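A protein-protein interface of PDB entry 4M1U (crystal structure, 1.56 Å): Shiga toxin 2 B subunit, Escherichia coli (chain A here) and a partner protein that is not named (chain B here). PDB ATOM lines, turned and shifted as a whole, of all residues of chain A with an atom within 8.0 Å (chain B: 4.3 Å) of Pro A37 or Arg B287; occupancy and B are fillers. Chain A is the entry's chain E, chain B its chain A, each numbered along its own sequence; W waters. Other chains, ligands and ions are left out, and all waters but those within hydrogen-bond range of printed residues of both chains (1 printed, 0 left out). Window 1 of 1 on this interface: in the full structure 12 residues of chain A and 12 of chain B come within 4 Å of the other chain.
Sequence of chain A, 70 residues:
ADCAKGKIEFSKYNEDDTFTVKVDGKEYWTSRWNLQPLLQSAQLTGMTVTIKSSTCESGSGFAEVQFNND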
ATOM      1  N   PHE A  19       6.440 -15.973  17.170  1.00  0.00           N
ATOM      2  CA  PHE A  19       7.705 -16.388  17.768  1.00  0.00           C
ATOM      3  C   PHE A  19       7.897 -15.628  19.079  1.00  0.00           C
ATOM      4  O   PHE A  19       8.045 -14.408  19.073  1.00  0.00           O
ATOM      5  CB  PHE A  19       8.859 -16.119  16.792  1.00  0.00           C
ATOM      6  CG  PHE A  19      10.170 -16.766  17.183  1.00  0.00           C
ATOM      7  CD1 PHE A  19      10.404 -18.117  16.924  1.00  0.00           C
ATOM      8  CD2 PHE A  19      11.183 -16.011  17.772  1.00  0.00           C
ATOM      9  CE1 PHE A  19      11.617 -18.712  17.270  1.00  0.00           C
ATOM     10  CE2 PHE A  19      12.405 -16.595  18.124  1.00  0.00           C
ATOM     11  CZ  PHE A  19      12.625 -17.948  17.867  1.00  0.00           C
ATOM     12  N   ARG A  32       7.580 -11.535  12.583  1.00  0.00           N
ATOM     13  CA  ARG A  32       8.587 -11.273  11.556  1.00  0.00           C
ATOM     14  C   ARG A  32       9.526 -12.473  11.474  1.00  0.00           C
ATOM     15  O   ARG A  32      10.288 -12.734  12.410  1.00  0.00           O
ATOM     16  CB  ARG A  32       9.391  -9.997  11.856  1.00  0.00           C
ATOM     17  CG  ARG A  32       8.571  -8.739  12.164  1.00  0.00           C
ATOM     18  CD  ARG A  32       7.934  -8.135  10.927  1.00  0.00           C
ATOM     19  NE  ARG A  32       6.972  -7.091  11.290  1.00  0.00           N
ATOM     20  CZ  ARG A  32       7.209  -5.784  11.221  1.00  0.00           C
ATOM     21  NH1 ARG A  32       8.379  -5.330  10.794  1.00  0.00           N
ATOM     22  NH2 ARG A  32       6.268  -4.923  11.580  1.00  0.00           N
ATOM     23  N   TRP A  33       9.467 -13.214  10.368  1.00  0.00           N
ATOM     24  CA  TRP A  33      10.377 -14.351  10.189  1.00  0.00           C
ATOM     25  C   TRP A  33      11.837 -13.910  10.139  1.00  0.00           C
ATOM     26  O   TRP A  33      12.720 -14.666  10.540  1.00  0.00           O
ATOM     27  CB  TRP A  33      10.031 -15.159   8.938  1.00  0.00           C
ATOM     28  CG  TRP A  33       8.949 -16.185   9.145  1.00  0.00           C
ATOM     29  CD1 TRP A  33       7.903 -16.121  10.031  1.00  0.00           C
ATOM     30  CD2 TRP A  33       8.790 -17.418   8.428  1.00  0.00           C
ATOM     31  NE1 TRP A  33       7.112 -17.242   9.910  1.00  0.00           N
ATOM     32  CE2 TRP A  33       7.634 -18.054   8.936  1.00  0.00           C
ATOM     33  CE3 TRP A  33       9.515 -18.047   7.406  1.00  0.00           C
ATOM     34  CZ2 TRP A  33       7.185 -19.293   8.460  1.00  0.00           C
ATOM     35  CZ3 TRP A  33       9.067 -19.281   6.928  1.00  0.00           C
ATOM     36  CH2 TRP A  33       7.910 -19.888   7.458  1.00  0.00           C
ATOM     37  N   ASN A  34      12.095 -12.689   9.659  1.00  0.00           N
ATOM     38  CA  ASN A  34      13.453 -12.143   9.679  1.00  0.00           C
ATOM     39  C   ASN A  34      14.079 -12.249  11.065  1.00  0.00           C
ATOM     40  O   ASN A  34      15.279 -12.510  11.196  1.00  0.00           O
ATOM     41  CB  ASN A  34      13.468 -10.665   9.269  1.00  0.00           C
ATOM     42  CG  ASN A  34      13.424 -10.461   7.768  1.00  0.00           C
ATOM     43  OD1 ASN A  34      13.705 -11.372   6.987  1.00  0.00           O
ATOM     44  ND2 ASN A  34      13.087  -9.242   7.355  1.00  0.00           N
ATOM     45  N   LEU A  35      13.255 -12.033  12.088  1.00  0.00           N
ATOM     46  CA  LEU A  35      13.727 -11.999  13.467  1.00  0.00           C
ATOM     47  C   LEU A  35      14.009 -13.374  14.063  1.00  0.00           C
ATOM     48  O   LEU A  35      14.738 -13.476  15.042  1.00  0.00           O
ATOM     49  CB  LEU A  35      12.753 -11.214  14.352  1.00  0.00           C
ATOM     50  CG  LEU A  35      12.990  -9.703  14.317  1.00  0.00           C
ATOM     51  CD1 LEU A  35      11.866  -8.960  15.029  1.00  0.00           C
ATOM     52  CD2 LEU A  35      14.347  -9.367  14.935  1.00  0.00           C
ATOM     53  N   GLN A  36      13.456 -14.431  13.475  1.00  0.00           N
ATOM     54  CA  GLN A  36      13.636 -15.767  14.057  1.00  0.00           C
ATOM     55  C   GLN A  36      15.103 -16.225  14.116  1.00  0.00           C
ATOM     56  O   GLN A  36      15.590 -16.543  15.203  1.00  0.00           O
ATOM     57  CB  GLN A  36      12.720 -16.805  13.403  1.00  0.00           C
ATOM     58  CG  GLN A  36      11.259 -16.538  13.703  1.00  0.00           C
ATOM     59  CD  GLN A  36      10.346 -17.678  13.303  1.00  0.00           C
ATOM     60  OE1 GLN A  36      10.766 -18.834  13.214  1.00  0.00           O
ATOM     61  NE2 GLN A  36       9.075 -17.357  13.080  1.00  0.00           N
ATOM     62  N   PRO A  37      15.819 -16.230  12.972  1.00  0.00           N
ATOM     63  CA  PRO A  37      17.230 -16.617  13.062  1.00  0.00           C
ATOM     64  C   PRO A  37      18.062 -15.632  13.879  1.00  0.00           C
ATOM     65  O   PRO A  37      18.970 -16.050  14.598  1.00  0.00           O
ATOM     66  CB  PRO A  37      17.694 -16.630  11.599  1.00  0.00           C
ATOM     67  CG  PRO A  37      16.684 -15.818  10.856  1.00  0.00           C
ATOM     68  CD  PRO A  37      15.398 -16.042  11.569  1.00  0.00           C
ATOM     69  N   LEU A  38      17.744 -14.344  13.778  1.00  0.00           N
ATOM     70  CA  LEU A  38      18.463 -13.316  14.533  1.00  0.00           C
ATOM     71  C   LEU A  38      18.287 -13.510  16.034  1.00  0.00           C
ATOM     72  O   LEU A  38      19.265 -13.481  16.790  1.00  0.00           O
ATOM     73  CB  LEU A  38      18.018 -11.916  14.108  1.00  0.00           C
ATOM     74  CG  LEU A  38      18.209 -11.551  12.629  1.00  0.00           C
ATOM     75  CD1 LEU A  38      17.552 -10.205  12.341  1.00  0.00           C
ATOM     76  CD2 LEU A  38      19.675 -11.537  12.205  1.00  0.00           C
ATOM     77  N   LEU A  39      17.045 -13.726  16.462  1.00  0.00           N
ATOM     78  CA  LEU A  39      16.770 -13.934  17.878  1.00  0.00           C
ATOM     79  C   LEU A  39      17.333 -15.249  18.397  1.00  0.00           C
ATOM     80  O   LEU A  39      17.881 -15.290  19.498  1.00  0.00           O
ATOM     81  CB  LEU A  39      15.271 -13.833  18.178  1.00  0.00           C
ATOM     82  CG  LEU A  39      14.662 -12.428  18.090  1.00  0.00           C
ATOM     83  CD1 LEU A  39      13.152 -12.536  18.033  1.00  0.00           C
ATOM     84  CD2 LEU A  39      15.102 -11.546  19.259  1.00  0.00           C
ATOM     85  N   GLN A  40      17.215 -16.322  17.613  1.00  0.00           N
ATOM     86  CA  GLN A  40      17.763 -17.603  18.067  1.00  0.00           C
ATOM     87  C   GLN A  40      19.288 -17.559  18.151  1.00  0.00           C
ATOM     88  O   GLN A  40      19.869 -18.087  19.101  1.00  0.00           O
ATOM     89  CB  GLN A  40      17.310 -18.780  17.206  1.00  0.00           C
ATOM     90  CG  GLN A  40      17.540 -20.111  17.928  1.00  0.00           C
ATOM     91  CD  GLN A  40      17.783 -21.268  16.991  1.00  0.00           C
ATOM     92  OE1 GLN A  40      18.439 -21.126  15.956  1.00  0.00           O
ATOM     93  NE2 GLN A  40      17.268 -22.434  17.359  1.00  0.00           N
ATOM     94  N   SER A  41      19.929 -16.922  17.171  1.00  0.00           N
ATOM     95  CA  SER A  41      21.385 -16.749  17.218  1.00  0.00           C
ATOM     96  C   SER A  41      21.789 -15.944  18.449  1.00  0.00           C
ATOM     97  O   SER A  41      22.767 -16.279  19.112  1.00  0.00           O
ATOM     98  CB  SER A  41      21.921 -16.104  15.938  1.00  0.00           C
ATOM     99  OG  SER A  41      21.755 -16.980  14.836  1.00  0.00           O
ATOM    100  N   ALA A  42      21.022 -14.899  18.758  1.00  0.00           N
ATOM    101  CA  ALA A  42      21.249 -14.108  19.969  1.00  0.00           C
ATOM    102  C   ALA A  42      21.104 -14.976  21.217  1.00  0.00           C
ATOM    103  O   ALA A  42      21.919 -14.884  22.139  1.00  0.00           O
ATOM    104  CB  ALA A  42      20.296 -12.923  20.019  1.00  0.00           C
ATOM    105  N   GLN A  43      20.079 -15.832  21.233  1.00  0.00           N
ATOM    106  CA  GLN A  43      19.853 -16.737  22.355  1.00  0.00           C
ATOM    107  C   GLN A  43      21.031 -17.692  22.563  1.00  0.00           C
ATOM    108  O   GLN A  43      21.544 -17.817  23.679  1.00  0.00           O
ATOM    109  CB  GLN A  43      18.556 -17.534  22.169  1.00  0.00           C
ATOM    110  CG  GLN A  43      18.249 -18.491  23.322  1.00  0.00           C
ATOM    111  CD  GLN A  43      17.064 -19.387  23.043  1.00  0.00           C
ATOM    112  OE1 GLN A  43      16.394 -19.252  22.012  1.00  0.00           O
ATOM    113  NE2 GLN A  43      16.794 -20.313  23.963  1.00  0.00           N
ATOM    114  N   LEU A  44      21.462 -18.355  21.493  1.00  0.00           N
ATOM    115  CA  LEU A  44      22.488 -19.388  21.621  1.00  0.00           C
ATOM    116  C   LEU A  44      23.901 -18.844  21.856  1.00  0.00           C
ATOM    117  O   LEU A  44      24.754 -19.566  22.358  1.00  0.00           O
ATOM    118  CB  LEU A  44      22.439 -20.365  20.437  1.00  0.00           C
ATOM    119  CG  LEU A  44      22.893 -19.918  19.047  1.00  0.00           C
ATOM    120  CD1 LEU A  44      24.383 -20.198  18.838  1.00  0.00           C
ATOM    121  CD2 LEU A  44      22.067 -20.650  17.999  1.00  0.00           C
ATOM    122  N   PHE A  67      20.709  -5.646  19.367  1.00  0.00           N
ATOM    123  CA  PHE A  67      21.578  -6.768  19.708  1.00  0.00           C
ATOM    124  C   PHE A  67      22.955  -6.245  20.112  1.00  0.00           C
ATOM    125  O   PHE A  67      23.574  -5.481  19.367  1.00  0.00           O
ATOM    126  CB  PHE A  67      21.738  -7.701  18.498  1.00  0.00           C
ATOM    127  CG  PHE A  67      20.445  -8.275  17.992  1.00  0.00           C
ATOM    128  CD1 PHE A  67      19.671  -7.582  17.060  1.00  0.00           C
ATOM    129  CD2 PHE A  67      20.006  -9.518  18.432  1.00  0.00           C
ATOM    130  CE1 PHE A  67      18.468  -8.116  16.588  1.00  0.00           C
ATOM    131  CE2 PHE A  67      18.810 -10.060  17.965  1.00  0.00           C
ATOM    132  CZ  PHE A  67      18.040  -9.357  17.044  1.00  0.00           C
ATOM    133  N   ALA B 283      26.069 -23.037  14.440  1.00  0.00           N
ATOM    134  CA  ALA B 283      24.657 -22.797  14.747  1.00  0.00           C
ATOM    135  C   ALA B 283      24.162 -21.394  14.385  1.00  0.00           C
ATOM    136  O   ALA B 283      22.955 -21.149  14.378  1.00  0.00           O
ATOM    137  CB  ALA B 283      24.374 -23.102  16.208  1.00  0.00           C
ATOM    138  N   PHE B 284      25.079 -20.471  14.092  1.00  0.00           N
ATOM    139  CA  PHE B 284      24.659 -19.201  13.489  1.00  0.00           C
ATOM    140  C   PHE B 284      25.141 -19.017  12.049  1.00  0.00           C
ATOM    141  O   PHE B 284      24.818 -18.011  11.411  1.00  0.00           O
ATOM    142  CB  PHE B 284      24.953 -17.973  14.377  1.00  0.00           C
ATOM    143  CG  PHE B 284      26.418 -17.677  14.603  1.00  0.00           C
ATOM    144  CD1 PHE B 284      27.158 -16.957  13.666  1.00  0.00           C
ATOM    145  CD2 PHE B 284      27.039 -18.065  15.787  1.00  0.00           C
ATOM    146  CE1 PHE B 284      28.505 -16.654  13.892  1.00  0.00           C
ATOM    147  CE2 PHE B 284      28.383 -17.757  16.030  1.00  0.00           C
ATOM    148  CZ  PHE B 284      29.118 -17.055  15.073  1.00  0.00           C
ATOM    149  N   LEU B 285      25.879 -20.000  11.535  1.00  0.00           N
ATOM    150  CA  LEU B 285      26.327 -19.975  10.137  1.00  0.00           C
ATOM    151  C   LEU B 285      25.561 -20.958   9.241  1.00  0.00           C
ATOM    152  O   LEU B 285      26.008 -21.272   8.132  1.00  0.00           O
ATOM    153  CB  LEU B 285      27.848 -20.204  10.028  1.00  0.00           C
ATOM    154  CG  LEU B 285      28.730 -19.207  10.789  1.00  0.00           C
ATOM    155  CD1 LEU B 285      30.171 -19.684  10.846  1.00  0.00           C
ATOM    156  CD2 LEU B 285      28.641 -17.790  10.199  1.00  0.00           C
ATOM    157  N   ASN B 286      24.418 -21.442   9.723  1.00  0.00           N
ATOM    158  CA  ASN B 286      23.609 -22.399   8.977  1.00  0.00           C
ATOM    159  C   ASN B 286      22.326 -21.787   8.422  1.00  0.00           C
ATOM    160  O   ASN B 286      21.376 -22.506   8.120  1.00  0.00           O
ATOM    161  CB  ASN B 286      23.276 -23.613   9.850  1.00  0.00           C
ATOM    162  CG  ASN B 286      22.351 -23.271  10.994  1.00  0.00           C
ATOM    163  OD1 ASN B 286      22.154 -22.098  11.320  1.00  0.00           O
ATOM    164  ND2 ASN B 286      21.775 -24.297  11.619  1.00  0.00           N
ATOM    165  N   ARG B 287      22.306 -20.464   8.296  1.00  0.00           N
ATOM    166  CA  ARG B 287      21.142 -19.756   7.767  1.00  0.00           C
ATOM    167  C   ARG B 287      21.285 -19.556   6.263  1.00  0.00           C
ATOM    168  O   ARG B 287      22.381 -19.288   5.772  1.00  0.00           O
ATOM    169  CB  ARG B 287      20.983 -18.403   8.458  1.00  0.00           C
ATOM    170  CG  ARG B 287      20.366 -18.467   9.851  1.00  0.00           C
ATOM    171  CD  ARG B 287      21.351 -18.895  10.941  1.00  0.00           C
ATOM    172  NE  ARG B 287      20.794 -18.625  12.268  1.00  0.00           N
ATOM    173  CZ  ARG B 287      20.231 -19.531  13.070  1.00  0.00           C
ATOM    174  NH1 ARG B 287      20.153 -20.812  12.719  1.00  0.00           N
ATOM    175  NH2 ARG B 287      19.745 -19.149  14.240  1.00  0.00           N
ATOM    176  N   LYS B 288      20.184 -19.698   5.528  1.00  0.00           N
ATOM    177  CA  LYS B 288      20.220 -19.383   4.099  1.00  0.00           C
ATOM    178  C   LYS B 288      19.996 -17.888   3.893  1.00  0.00           C
ATOM    179  O   LYS B 288      19.881 -17.136   4.864  1.00  0.00           O
ATOM    180  CB  LYS B 288      19.219 -20.230   3.296  1.00  0.00           C
ATOM    181  CG  LYS B 288      17.754 -19.957   3.588  1.00  0.00           C
ATOM    182  CD  LYS B 288      16.890 -20.742   2.609  1.00  0.00           C
ATOM    183  CE  LYS B 288      15.423 -20.463   2.827  1.00  0.00           C
ATOM    184  NZ  LYS B 288      14.570 -21.253   1.894  1.00  0.00           N
ATOM    185  N   GLN B 290      18.537 -14.445   3.661  1.00  0.00           N
ATOM    186  CA  GLN B 290      17.458 -13.927   4.500  1.00  0.00           C
ATOM    187  C   GLN B 290      16.179 -13.655   3.704  1.00  0.00           C
ATOM    188  O   GLN B 290      15.082 -13.994   4.150  1.00  0.00           O
ATOM    189  CB  GLN B 290      17.917 -12.664   5.229  1.00  0.00           C
ATOM    190  CG  GLN B 290      16.915 -12.093   6.233  1.00  0.00           C
ATOM    191  CD  GLN B 290      16.907 -12.811   7.573  1.00  0.00           C
ATOM    192  OE1 GLN B 290      17.050 -14.035   7.647  1.00  0.00           O
ATOM    193  NE2 GLN B 290      16.716 -12.047   8.643  1.00  0.00           N
ATOM    194  N   TYR B 293      14.584 -16.935   2.976  1.00  0.00           N
ATOM    195  CA  TYR B 293      14.044 -17.530   4.194  1.00  0.00           C
ATOM    196  C   TYR B 293      12.655 -16.984   4.515  1.00  0.00           C
ATOM    197  O   TYR B 293      11.706 -17.747   4.707  1.00  0.00           O
ATOM    198  CB  TYR B 293      15.006 -17.278   5.355  1.00  0.00           C
ATOM    199  CG  TYR B 293      14.542 -17.793   6.694  1.00  0.00           C
ATOM    200  CD1 TYR B 293      14.606 -19.152   7.004  1.00  0.00           C
ATOM    201  CD2 TYR B 293      14.074 -16.913   7.665  1.00  0.00           C
ATOM    202  CE1 TYR B 293      14.199 -19.621   8.248  1.00  0.00           C
ATOM    203  CE2 TYR B 293      13.659 -17.367   8.908  1.00  0.00           C
ATOM    204  CZ  TYR B 293      13.730 -18.721   9.198  1.00  0.00           C
ATOM    205  OH  TYR B 293      13.327 -19.158  10.434  1.00  0.00           O
HETATM  206  O   HOH W   1      21.636 -15.606  12.512  1.00  0.00           O
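Among the printed residues, pairs that only touch across the chains: Trp A33 with Tyr B293 (3.3 Å), Gln A36 with Tyr B293 (3.8 Å), Pro A37 with Gln B290 (3.7 Å), Pro A37 with Tyr B293 (3.4 Å), Ser A41 with Phe B284 (3.4 Å) and Leu A44 with Ala B283 (3.8 Å).
Water W1 lies within hydrogen-bond range of OG of Ser A41, NE of Arg B287 and O of Pro A37.
Of chain B, only Arg B287 (3.2 Å), Gln B290 (3.7 Å) and Tyr B293 (3.4 Å) come within 4 Å of Pro A37. Of chain A, only Pro A37 (3.2 Å), Gln A40 (2.9 Å) and Ser A41 (3.0 Å) come within 4 Å of Arg B287. Of the printed residues of chain B, Trp A33 touches Tyr B293 (3.3 Å). Of the printed residues of chain A, Phe B284 touches Ser A41. Of the printed residues of chain B, Ser A41 touches Phe B284 (3.4 Å) and Arg B287 (3.0 Å). Printed residues of chain B within 4 Å of Gln A40: Arg B287. The nearest residue of chain A that does not touch Arg B287 is Leu A44 (4.7 Å). The nearest printed residue of chain A that does not touch Tyr B293 is Asn A34 (5.0 Å).
Of the 8 printed residues of chain B, 5 touch a printed residue of chain A. Printed residues of chain B that touch a printed residue of chain A: Ala B283, Phe B284, Arg B287, Gln B290 and Tyr B293. Hydrophobic or aromatic side chains of chain B within 4 Å of the printed part of chain A: Ala B283, Phe B284 and Tyr B293. Of the 15 printed residues of chain A, 7 touch a printed residue of chain B. Among the printed residues, 10 pairs touch across the chains. Among the printed residues, no Asp or Glu carboxylate lies within 4 Å of a Lys or Arg side-chain nitrogen of the other chain.
The backbone carbonyl oxygen (O) of Pro A37 lies within hydrogen-bond range of the guanidinium group (NH2) of Arg B287 (3.2 Å). OE1 of Gln A40 is in hydrogen-bond range of NH2 of Arg B287, at 2.9 Å. The guanidinium group of Arg B287 lies within hydrogen-bond range of the side-chain hydroxyl of Ser A41 (3.0 Å). NE2 of Gln B290 sits at hydrogen-bond distance from O of Asn A34, 3.0 Å away.
The backbone carbonyl oxygen (O) of Ala B283 lies close to the side-chain amide oxygen (OD1) of Asn B286 (3.3 Å). The backbone carbonyl oxygen of Ala B283 is in hydrogen-bond range of the guanidinium group of Arg B287 (3.3 Å). OD1 of Asn B286 sits at hydrogen-bond distance from NH1 of Arg B287, at 2.8 Å. The side-chain hydroxyl (OG) of Ser A41 sits at hydrogen-bond distance from the backbone carbonyl oxygen (O) of Pro A37.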
